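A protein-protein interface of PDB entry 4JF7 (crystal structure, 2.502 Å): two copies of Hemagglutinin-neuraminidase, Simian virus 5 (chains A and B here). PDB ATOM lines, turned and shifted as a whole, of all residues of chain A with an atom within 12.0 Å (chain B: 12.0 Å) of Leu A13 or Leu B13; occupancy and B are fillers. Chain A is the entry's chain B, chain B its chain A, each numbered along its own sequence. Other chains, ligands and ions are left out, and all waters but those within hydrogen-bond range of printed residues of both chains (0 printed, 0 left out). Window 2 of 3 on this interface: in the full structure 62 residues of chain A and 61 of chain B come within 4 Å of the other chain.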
ATOM      1  N   LEU A  13     -16.358   4.388 -16.672  1.00  0.00           N
ATOM      2  CA  LEU A  13     -16.859   3.312 -17.520  1.00  0.00           C
ATOM      3  C   LEU A  13     -15.826   3.036 -18.619  1.00  0.00           C
ATOM      4  O   LEU A  13     -16.050   2.212 -19.510  1.00  0.00           O
ATOM      5  CB  LEU A  13     -18.233   3.685 -18.091  1.00  0.00           C
ATOM      6  CG  LEU A  13     -19.130   2.619 -18.732  1.00  0.00           C
ATOM      7  CD1 LEU A  13     -20.494   2.597 -18.133  1.00  0.00           C
ATOM      8  CD2 LEU A  13     -19.268   2.958 -20.178  1.00  0.00           C
ATOM      9  N   ASN A  14     -14.694   3.739 -18.520  1.00  0.00           N
ATOM     10  CA  ASN A  14     -13.494   3.502 -19.323  1.00  0.00           C
ATOM     11  C   ASN A  14     -12.435   2.802 -18.467  1.00  0.00           C
ATOM     12  O   ASN A  14     -11.494   2.197 -18.985  1.00  0.00           O
ATOM     13  CB  ASN A  14     -12.947   4.835 -19.856  1.00  0.00           C
ATOM     14  CG  ASN A  14     -11.909   4.659 -20.967  1.00  0.00           C
ATOM     15  OD1 ASN A  14     -11.785   3.590 -21.568  1.00  0.00           O
ATOM     16  ND2 ASN A  14     -11.174   5.725 -21.255  1.00  0.00           N
ATOM     17  N   ASN A  15     -12.600   2.899 -17.150  1.00  0.00           N
ATOM     18  CA  ASN A  15     -11.720   2.227 -16.199  1.00  0.00           C
ATOM     19  C   ASN A  15     -11.988   0.724 -16.155  1.00  0.00           C
ATOM     20  O   ASN A  15     -11.262  -0.029 -15.506  1.00  0.00           O
ATOM     21  CB  ASN A  15     -11.877   2.831 -14.800  1.00  0.00           C
ATOM     22  N   ILE A  16     -13.038   0.296 -16.853  1.00  0.00           N
ATOM     23  CA  ILE A  16     -13.401  -1.116 -16.931  1.00  0.00           C
ATOM     24  C   ILE A  16     -12.724  -1.764 -18.142  1.00  0.00           C
ATOM     25  O   ILE A  16     -13.344  -2.487 -18.924  1.00  0.00           O
ATOM     26  CB  ILE A  16     -14.935  -1.309 -16.974  1.00  0.00           C
ATOM     27  CG1 ILE A  16     -15.614  -0.345 -15.996  1.00  0.00           C
ATOM     28  CG2 ILE A  16     -15.317  -2.747 -16.637  1.00  0.00           C
ATOM     29  CD1 ILE A  16     -15.196  -0.536 -14.547  1.00  0.00           C
ATOM     30  N   LEU A  17     -11.441  -1.457 -18.294  1.00  0.00           N
ATOM     31  CA  LEU A  17     -10.556  -2.160 -19.210  1.00  0.00           C
ATOM     32  C   LEU A  17      -9.201  -2.196 -18.524  1.00  0.00           C
ATOM     33  O   LEU A  17      -8.392  -3.094 -18.752  1.00  0.00           O
ATOM     34  CB  LEU A  17     -10.466  -1.450 -20.565  1.00  0.00           C
ATOM     35  CG  LEU A  17      -9.690  -2.192 -21.661  1.00  0.00           C
ATOM     36  CD1 LEU A  17     -10.468  -2.204 -22.969  1.00  0.00           C
ATOM     37  CD2 LEU A  17      -8.312  -1.582 -21.866  1.00  0.00           C
ATOM     38  N   SER A  18      -8.973  -1.204 -17.666  1.00  0.00           N
ATOM     39  CA  SER A  18      -7.806  -1.184 -16.799  1.00  0.00           C
ATOM     40  C   SER A  18      -7.917  -2.307 -15.768  1.00  0.00           C
ATOM     41  O   SER A  18      -6.922  -2.947 -15.425  1.00  0.00           O
ATOM     42  CB  SER A  18      -7.668   0.180 -16.113  1.00  0.00           C
ATOM     43  OG  SER A  18      -8.898   0.601 -15.546  1.00  0.00           O
ATOM     44  N   VAL A  19      -9.136  -2.543 -15.286  1.00  0.00           N
ATOM     45  CA  VAL A  19      -9.412  -3.666 -14.393  1.00  0.00           C
ATOM     46  C   VAL A  19      -9.583  -4.965 -15.180  1.00  0.00           C
ATOM     47  O   VAL A  19      -9.058  -6.007 -14.790  1.00  0.00           O
ATOM     48  CB  VAL A  19     -10.669  -3.416 -13.527  1.00  0.00           C
ATOM     49  CG1 VAL A  19     -11.321  -4.730 -13.135  1.00  0.00           C
ATOM     50  CG2 VAL A  19     -10.317  -2.599 -12.292  1.00  0.00           C
ATOM     51  N   ALA A  20     -10.305  -4.889 -16.297  1.00  0.00           N
ATOM     52  CA  ALA A  20     -10.586  -6.062 -17.127  1.00  0.00           C
ATOM     53  C   ALA A  20      -9.330  -6.680 -17.742  1.00  0.00           C
ATOM     54  O   ALA A  20      -9.281  -7.886 -17.982  1.00  0.00           O
ATOM     55  CB  ALA A  20     -11.592  -5.719 -18.213  1.00  0.00           C
ATOM     56  N   ASN A  21      -8.322  -5.853 -18.005  1.00  0.00           N
ATOM     57  CA  ASN A  21      -7.034  -6.362 -18.467  1.00  0.00           C
ATOM     58  C   ASN A  21      -6.248  -6.970 -17.313  1.00  0.00           C
ATOM     59  O   ASN A  21      -5.430  -7.868 -17.513  1.00  0.00           O
ATOM     60  CB  ASN A  21      -6.211  -5.263 -19.144  1.00  0.00           C
ATOM     61  CG  ASN A  21      -4.927  -5.791 -19.752  1.00  0.00           C
ATOM     62  OD1 ASN A  21      -4.955  -6.509 -20.750  1.00  0.00           O
ATOM     63  ND2 ASN A  21      -3.794  -5.440 -19.153  1.00  0.00           N
ATOM     64  N   ILE A  23      -7.842  -8.438 -14.840  1.00  0.00           N
ATOM     65  CA  ILE A  23      -8.571  -9.674 -14.574  1.00  0.00           C
ATOM     66  C   ILE A  23      -8.070 -10.799 -15.480  1.00  0.00           C
ATOM     67  O   ILE A  23      -7.774 -11.901 -15.009  1.00  0.00           O
ATOM     68  CB  ILE A  23     -10.091  -9.504 -14.761  1.00  0.00           C
ATOM     69  CG1 ILE A  23     -10.659  -8.548 -13.711  1.00  0.00           C
ATOM     70  CG2 ILE A  23     -10.794 -10.848 -14.661  1.00  0.00           C
ATOM     71  CD1 ILE A  23     -12.145  -8.279 -13.870  1.00  0.00           C
ATOM     72  N   ILE B   9     -28.050   5.203 -14.023  1.00  0.00           N
ATOM     73  CA  ILE B   9     -26.886   4.471 -14.512  1.00  0.00           C
ATOM     74  C   ILE B   9     -25.798   4.380 -13.437  1.00  0.00           C
ATOM     75  O   ILE B   9     -25.015   3.425 -13.409  1.00  0.00           O
ATOM     76  CB  ILE B   9     -26.337   5.099 -15.823  1.00  0.00           C
ATOM     77  CG1 ILE B   9     -26.603   4.167 -17.008  1.00  0.00           C
ATOM     78  CG2 ILE B   9     -24.849   5.438 -15.713  1.00  0.00           C
ATOM     79  CD1 ILE B   9     -28.071   3.899 -17.252  1.00  0.00           C
ATOM     80  N   THR B  10     -25.782   5.364 -12.542  1.00  0.00           N
ATOM     81  CA  THR B  10     -24.776   5.460 -11.484  1.00  0.00           C
ATOM     82  C   THR B  10     -24.682   4.210 -10.603  1.00  0.00           C
ATOM     83  O   THR B  10     -23.593   3.832 -10.165  1.00  0.00           O
ATOM     84  CB  THR B  10     -25.034   6.686 -10.585  1.00  0.00           C
ATOM     85  N   ASP B  11     -25.827   3.583 -10.340  1.00  0.00           N
ATOM     86  CA  ASP B  11     -25.876   2.356  -9.548  1.00  0.00           C
ATOM     87  C   ASP B  11     -25.061   1.260 -10.217  1.00  0.00           C
ATOM     88  O   ASP B  11     -24.179   0.659  -9.604  1.00  0.00           O
ATOM     89  CB  ASP B  11     -27.321   1.868  -9.398  1.00  0.00           C
ATOM     90  CG  ASP B  11     -28.210   2.870  -8.690  1.00  0.00           C
ATOM     91  OD1 ASP B  11     -27.813   4.048  -8.574  1.00  0.00           O
ATOM     92  OD2 ASP B  11     -29.316   2.478  -8.260  1.00  0.00           O
ATOM     93  N   LEU B  12     -25.365   1.013 -11.486  1.00  0.00           N
ATOM     94  CA  LEU B  12     -24.776  -0.099 -12.219  1.00  0.00           C
ATOM     95  C   LEU B  12     -23.490   0.295 -12.939  1.00  0.00           C
ATOM     96  O   LEU B  12     -23.164  -0.231 -14.002  1.00  0.00           O
ATOM     97  CB  LEU B  12     -25.811  -0.705 -13.166  1.00  0.00           C
ATOM     98  CG  LEU B  12     -26.958  -1.329 -12.361  1.00  0.00           C
ATOM     99  CD1 LEU B  12     -28.319  -0.829 -12.819  1.00  0.00           C
ATOM    100  CD2 LEU B  12     -26.892  -2.852 -12.404  1.00  0.00           C
ATOM    101  N   LEU B  13     -22.772   1.235 -12.335  1.00  0.00           N
ATOM    102  CA  LEU B  13     -21.415   1.573 -12.735  1.00  0.00           C
ATOM    103  C   LEU B  13     -20.510   1.430 -11.518  1.00  0.00           C
ATOM    104  O   LEU B  13     -19.541   0.668 -11.535  1.00  0.00           O
ATOM    105  CB  LEU B  13     -21.347   3.003 -13.273  1.00  0.00           C
ATOM    106  CG  LEU B  13     -21.364   3.173 -14.792  1.00  0.00           C
ATOM    107  CD1 LEU B  13     -22.636   2.588 -15.391  1.00  0.00           C
ATOM    108  CD2 LEU B  13     -21.196   4.641 -15.178  1.00  0.00           C
ATOM    109  N   ASN B  14     -20.844   2.160 -10.456  1.00  0.00           N
ATOM    110  CA  ASN B  14     -20.110   2.084  -9.197  1.00  0.00           C
ATOM    111  C   ASN B  14     -20.122   0.675  -8.608  1.00  0.00           C
ATOM    112  O   ASN B  14     -19.218   0.303  -7.858  1.00  0.00           O
ATOM    113  CB  ASN B  14     -20.667   3.091  -8.185  1.00  0.00           C
ATOM    114  N   ASN B  15     -21.151  -0.099  -8.950  1.00  0.00           N
ATOM    115  CA  ASN B  15     -21.251  -1.499  -8.536  1.00  0.00           C
ATOM    116  C   ASN B  15     -20.149  -2.371  -9.130  1.00  0.00           C
ATOM    117  O   ASN B  15     -19.444  -3.065  -8.400  1.00  0.00           O
ATOM    118  CB  ASN B  15     -22.621  -2.083  -8.899  1.00  0.00           C
ATOM    119  CG  ASN B  15     -23.662  -1.853  -7.818  1.00  0.00           C
ATOM    120  OD1 ASN B  15     -23.343  -1.804  -6.630  1.00  0.00           O
ATOM    121  ND2 ASN B  15     -24.918  -1.721  -8.228  1.00  0.00           N
ATOM    122  N   ILE B  16     -20.017  -2.331 -10.456  1.00  0.00           N
ATOM    123  CA  ILE B  16     -18.977  -3.072 -11.172  1.00  0.00           C
ATOM    124  C   ILE B  16     -17.581  -2.762 -10.629  1.00  0.00           C
ATOM    125  O   ILE B  16     -16.811  -3.681 -10.328  1.00  0.00           O
ATOM    126  CB  ILE B  16     -19.001  -2.776 -12.698  1.00  0.00           C
ATOM    127  CG1 ILE B  16     -20.119  -3.556 -13.396  1.00  0.00           C
ATOM    128  CG2 ILE B  16     -17.666  -3.123 -13.338  1.00  0.00           C
ATOM    129  CD1 ILE B  16     -20.038  -3.510 -14.922  1.00  0.00           C
ATOM    130  N   LEU B  17     -17.274  -1.471 -10.497  1.00  0.00           N
ATOM    131  CA  LEU B  17     -15.961  -1.017 -10.040  1.00  0.00           C
ATOM    132  C   LEU B  17     -15.504  -1.741  -8.778  1.00  0.00           C
ATOM    133  O   LEU B  17     -14.448  -2.374  -8.766  1.00  0.00           O
ATOM    134  CB  LEU B  17     -15.967   0.493  -9.792  1.00  0.00           C
ATOM    135  CG  LEU B  17     -14.619   1.080  -9.372  1.00  0.00           C
ATOM    136  CD1 LEU B  17     -13.928   1.752 -10.552  1.00  0.00           C
ATOM    137  CD2 LEU B  17     -14.770   2.041  -8.202  1.00  0.00           C
ATOM    138  N   SER B  18     -16.309  -1.657  -7.725  1.00  0.00           N
ATOM    139  CA  SER B  18     -15.974  -2.287  -6.455  1.00  0.00           C
ATOM    140  C   SER B  18     -16.136  -3.807  -6.498  1.00  0.00           C
ATOM    141  O   SER B  18     -15.619  -4.511  -5.630  1.00  0.00           O
ATOM    142  CB  SER B  18     -16.807  -1.686  -5.322  1.00  0.00           C
ATOM    143  OG  SER B  18     -16.569  -0.292  -5.211  1.00  0.00           O
ATOM    144  N   VAL B  19     -16.852  -4.305  -7.506  1.00  0.00           N
ATOM    145  CA  VAL B  19     -17.011  -5.748  -7.711  1.00  0.00           C
ATOM    146  C   VAL B  19     -15.878  -6.308  -8.570  1.00  0.00           C
ATOM    147  O   VAL B  19     -15.290  -7.346  -8.250  1.00  0.00           O
ATOM    148  CB  VAL B  19     -18.380  -6.101  -8.355  1.00  0.00           C
ATOM    149  CG1 VAL B  19     -18.327  -7.456  -9.067  1.00  0.00           C
ATOM    150  CG2 VAL B  19     -19.485  -6.087  -7.304  1.00  0.00           C
ATOM    151  N   ALA B  20     -15.572  -5.609  -9.660  1.00  0.00           N
ATOM    152  CA  ALA B  20     -14.455  -5.981 -10.518  1.00  0.00           C
ATOM    153  C   ALA B  20     -13.128  -5.755  -9.790  1.00  0.00           C
ATOM    154  O   ALA B  20     -12.101  -6.327 -10.160  1.00  0.00           O
ATOM    155  CB  ALA B  20     -14.503  -5.203 -11.821  1.00  0.00           C
ATOM    156  N   ASN B  21     -13.162  -4.917  -8.752  1.00  0.00           N
ATOM    157  CA  ASN B  21     -12.016  -4.730  -7.863  1.00  0.00           C
ATOM    158  C   ASN B  21     -11.799  -5.941  -6.956  1.00  0.00           C
ATOM    159  O   ASN B  21     -10.664  -6.351  -6.725  1.00  0.00           O
ATOM    160  CB  ASN B  21     -12.166  -3.459  -7.018  1.00  0.00           C
ATOM    161  CG  ASN B  21     -11.395  -2.282  -7.589  1.00  0.00           C
ATOM    162  OD1 ASN B  21     -10.324  -2.455  -8.174  1.00  0.00           O
ATOM    163  ND2 ASN B  21     -11.935  -1.075  -7.418  1.00  0.00           N
ATOM    164  N   GLN B  22     -12.891  -6.503  -6.442  1.00  0.00           N
ATOM    165  CA  GLN B  22     -12.817  -7.711  -5.624  1.00  0.00           C
ATOM    166  C   GLN B  22     -12.323  -8.890  -6.455  1.00  0.00           C
ATOM    167  O   GLN B  22     -11.739  -9.833  -5.926  1.00  0.00           O
ATOM    168  CB  GLN B  22     -14.178  -8.036  -5.006  1.00  0.00           C
ATOM    169  CG  GLN B  22     -14.656  -7.021  -3.983  1.00  0.00           C
ATOM    170  CD  GLN B  22     -16.094  -7.256  -3.561  1.00  0.00           C
ATOM    171  OE1 GLN B  22     -16.547  -8.399  -3.470  1.00  0.00           O
ATOM    172  NE2 GLN B  22     -16.823  -6.171  -3.311  1.00  0.00           N
ATOM    173  N   ILE B  23     -12.562  -8.822  -7.761  1.00  0.00           N
ATOM    174  CA  ILE B  23     -12.080  -9.836  -8.692  1.00  0.00           C
ATOM    175  C   ILE B  23     -10.570  -9.720  -8.890  1.00  0.00           C
ATOM    176  O   ILE B  23      -9.855 -10.727  -8.857  1.00  0.00           O
ATOM    177  CB  ILE B  23     -12.810  -9.741 -10.042  1.00  0.00           C
ATOM    178  CG1 ILE B  23     -14.291 -10.091  -9.850  1.00  0.00           C
ATOM    179  CG2 ILE B  23     -12.160 -10.657 -11.067  1.00  0.00           C
ATOM    180  CD1 ILE B  23     -15.170  -9.779 -11.037  1.00  0.00           C
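Among the printed residues, merely in contact across the chains: Leu A13 with Leu B13, Ile A16 with Ile B16, Val A19 with Ala B20 and Ile A23 with Ile B23.
Of chain A, only Leu A13 (3.5 Å) comes within 4 Å of Leu B13.
No residue of chain B comes within 4 Å of Asn A14.
No residue of chain B comes within 4 Å of Asn A15.
Ile A16 touches just one residue of chain B: Ile B16 (3.8 Å).
No residue of chain A comes within 4 Å of Thr B10.
No residue of chain A comes within 4 Å of Leu B12.
Ile B16 touches just one residue of chain A: Ile A16.
No residue of chain A comes within 4 Å of Leu B17.
Of the printed residues of chain B, Ile A23 touches Ile B23.
Of the printed residues of chain B, Val A19 touches Ala B20.
Of the printed residues of chain A, Ala B20 touches Val A19.
Of the printed residues of chain A, Ile B23 touches Ile A23 (3.7 Å).
Ser A18 touches none of the printed residues of chain B.
Asn A21 touches none of the printed residues of chain B.
The nearest residue of chain A that does not touch Leu B13 is Ile A16 (5.4 Å).
The nearest printed residue of chain A that does not touch Ile B23 is Val A19 (6.1 Å).
Of the 15 printed residues of chain B, 4 touch a printed residue of chain A.
Along chain B the printed residues that touch a printed residue of chain A span positions 13 to 23.
Of the 10 printed residues of chain A, 4 touch a printed residue of chain B.
Printed residues of chain A that touch a printed residue of chain B: Leu A13, Ile A16, Val A19 and Ile A23.
Among the printed residues, no Asp or Glu carboxylate lies within 4 Å of a Lys or Arg side-chain nitrogen of the other chain.
Leu B13 touches its own counterpart, Leu A13.
Ile A16 touches its own counterpart, Ile B16.
Val A19 touches Ala B20, but with the chains exchanged Ala A20 does not touch Val B19 (9.6 Å).
Ile A23 touches its own counterpart, Ile B23.
Of the 4 pairs that touch across the chains among the printed residues, 3 have their exchanged pair printed and touching as well.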
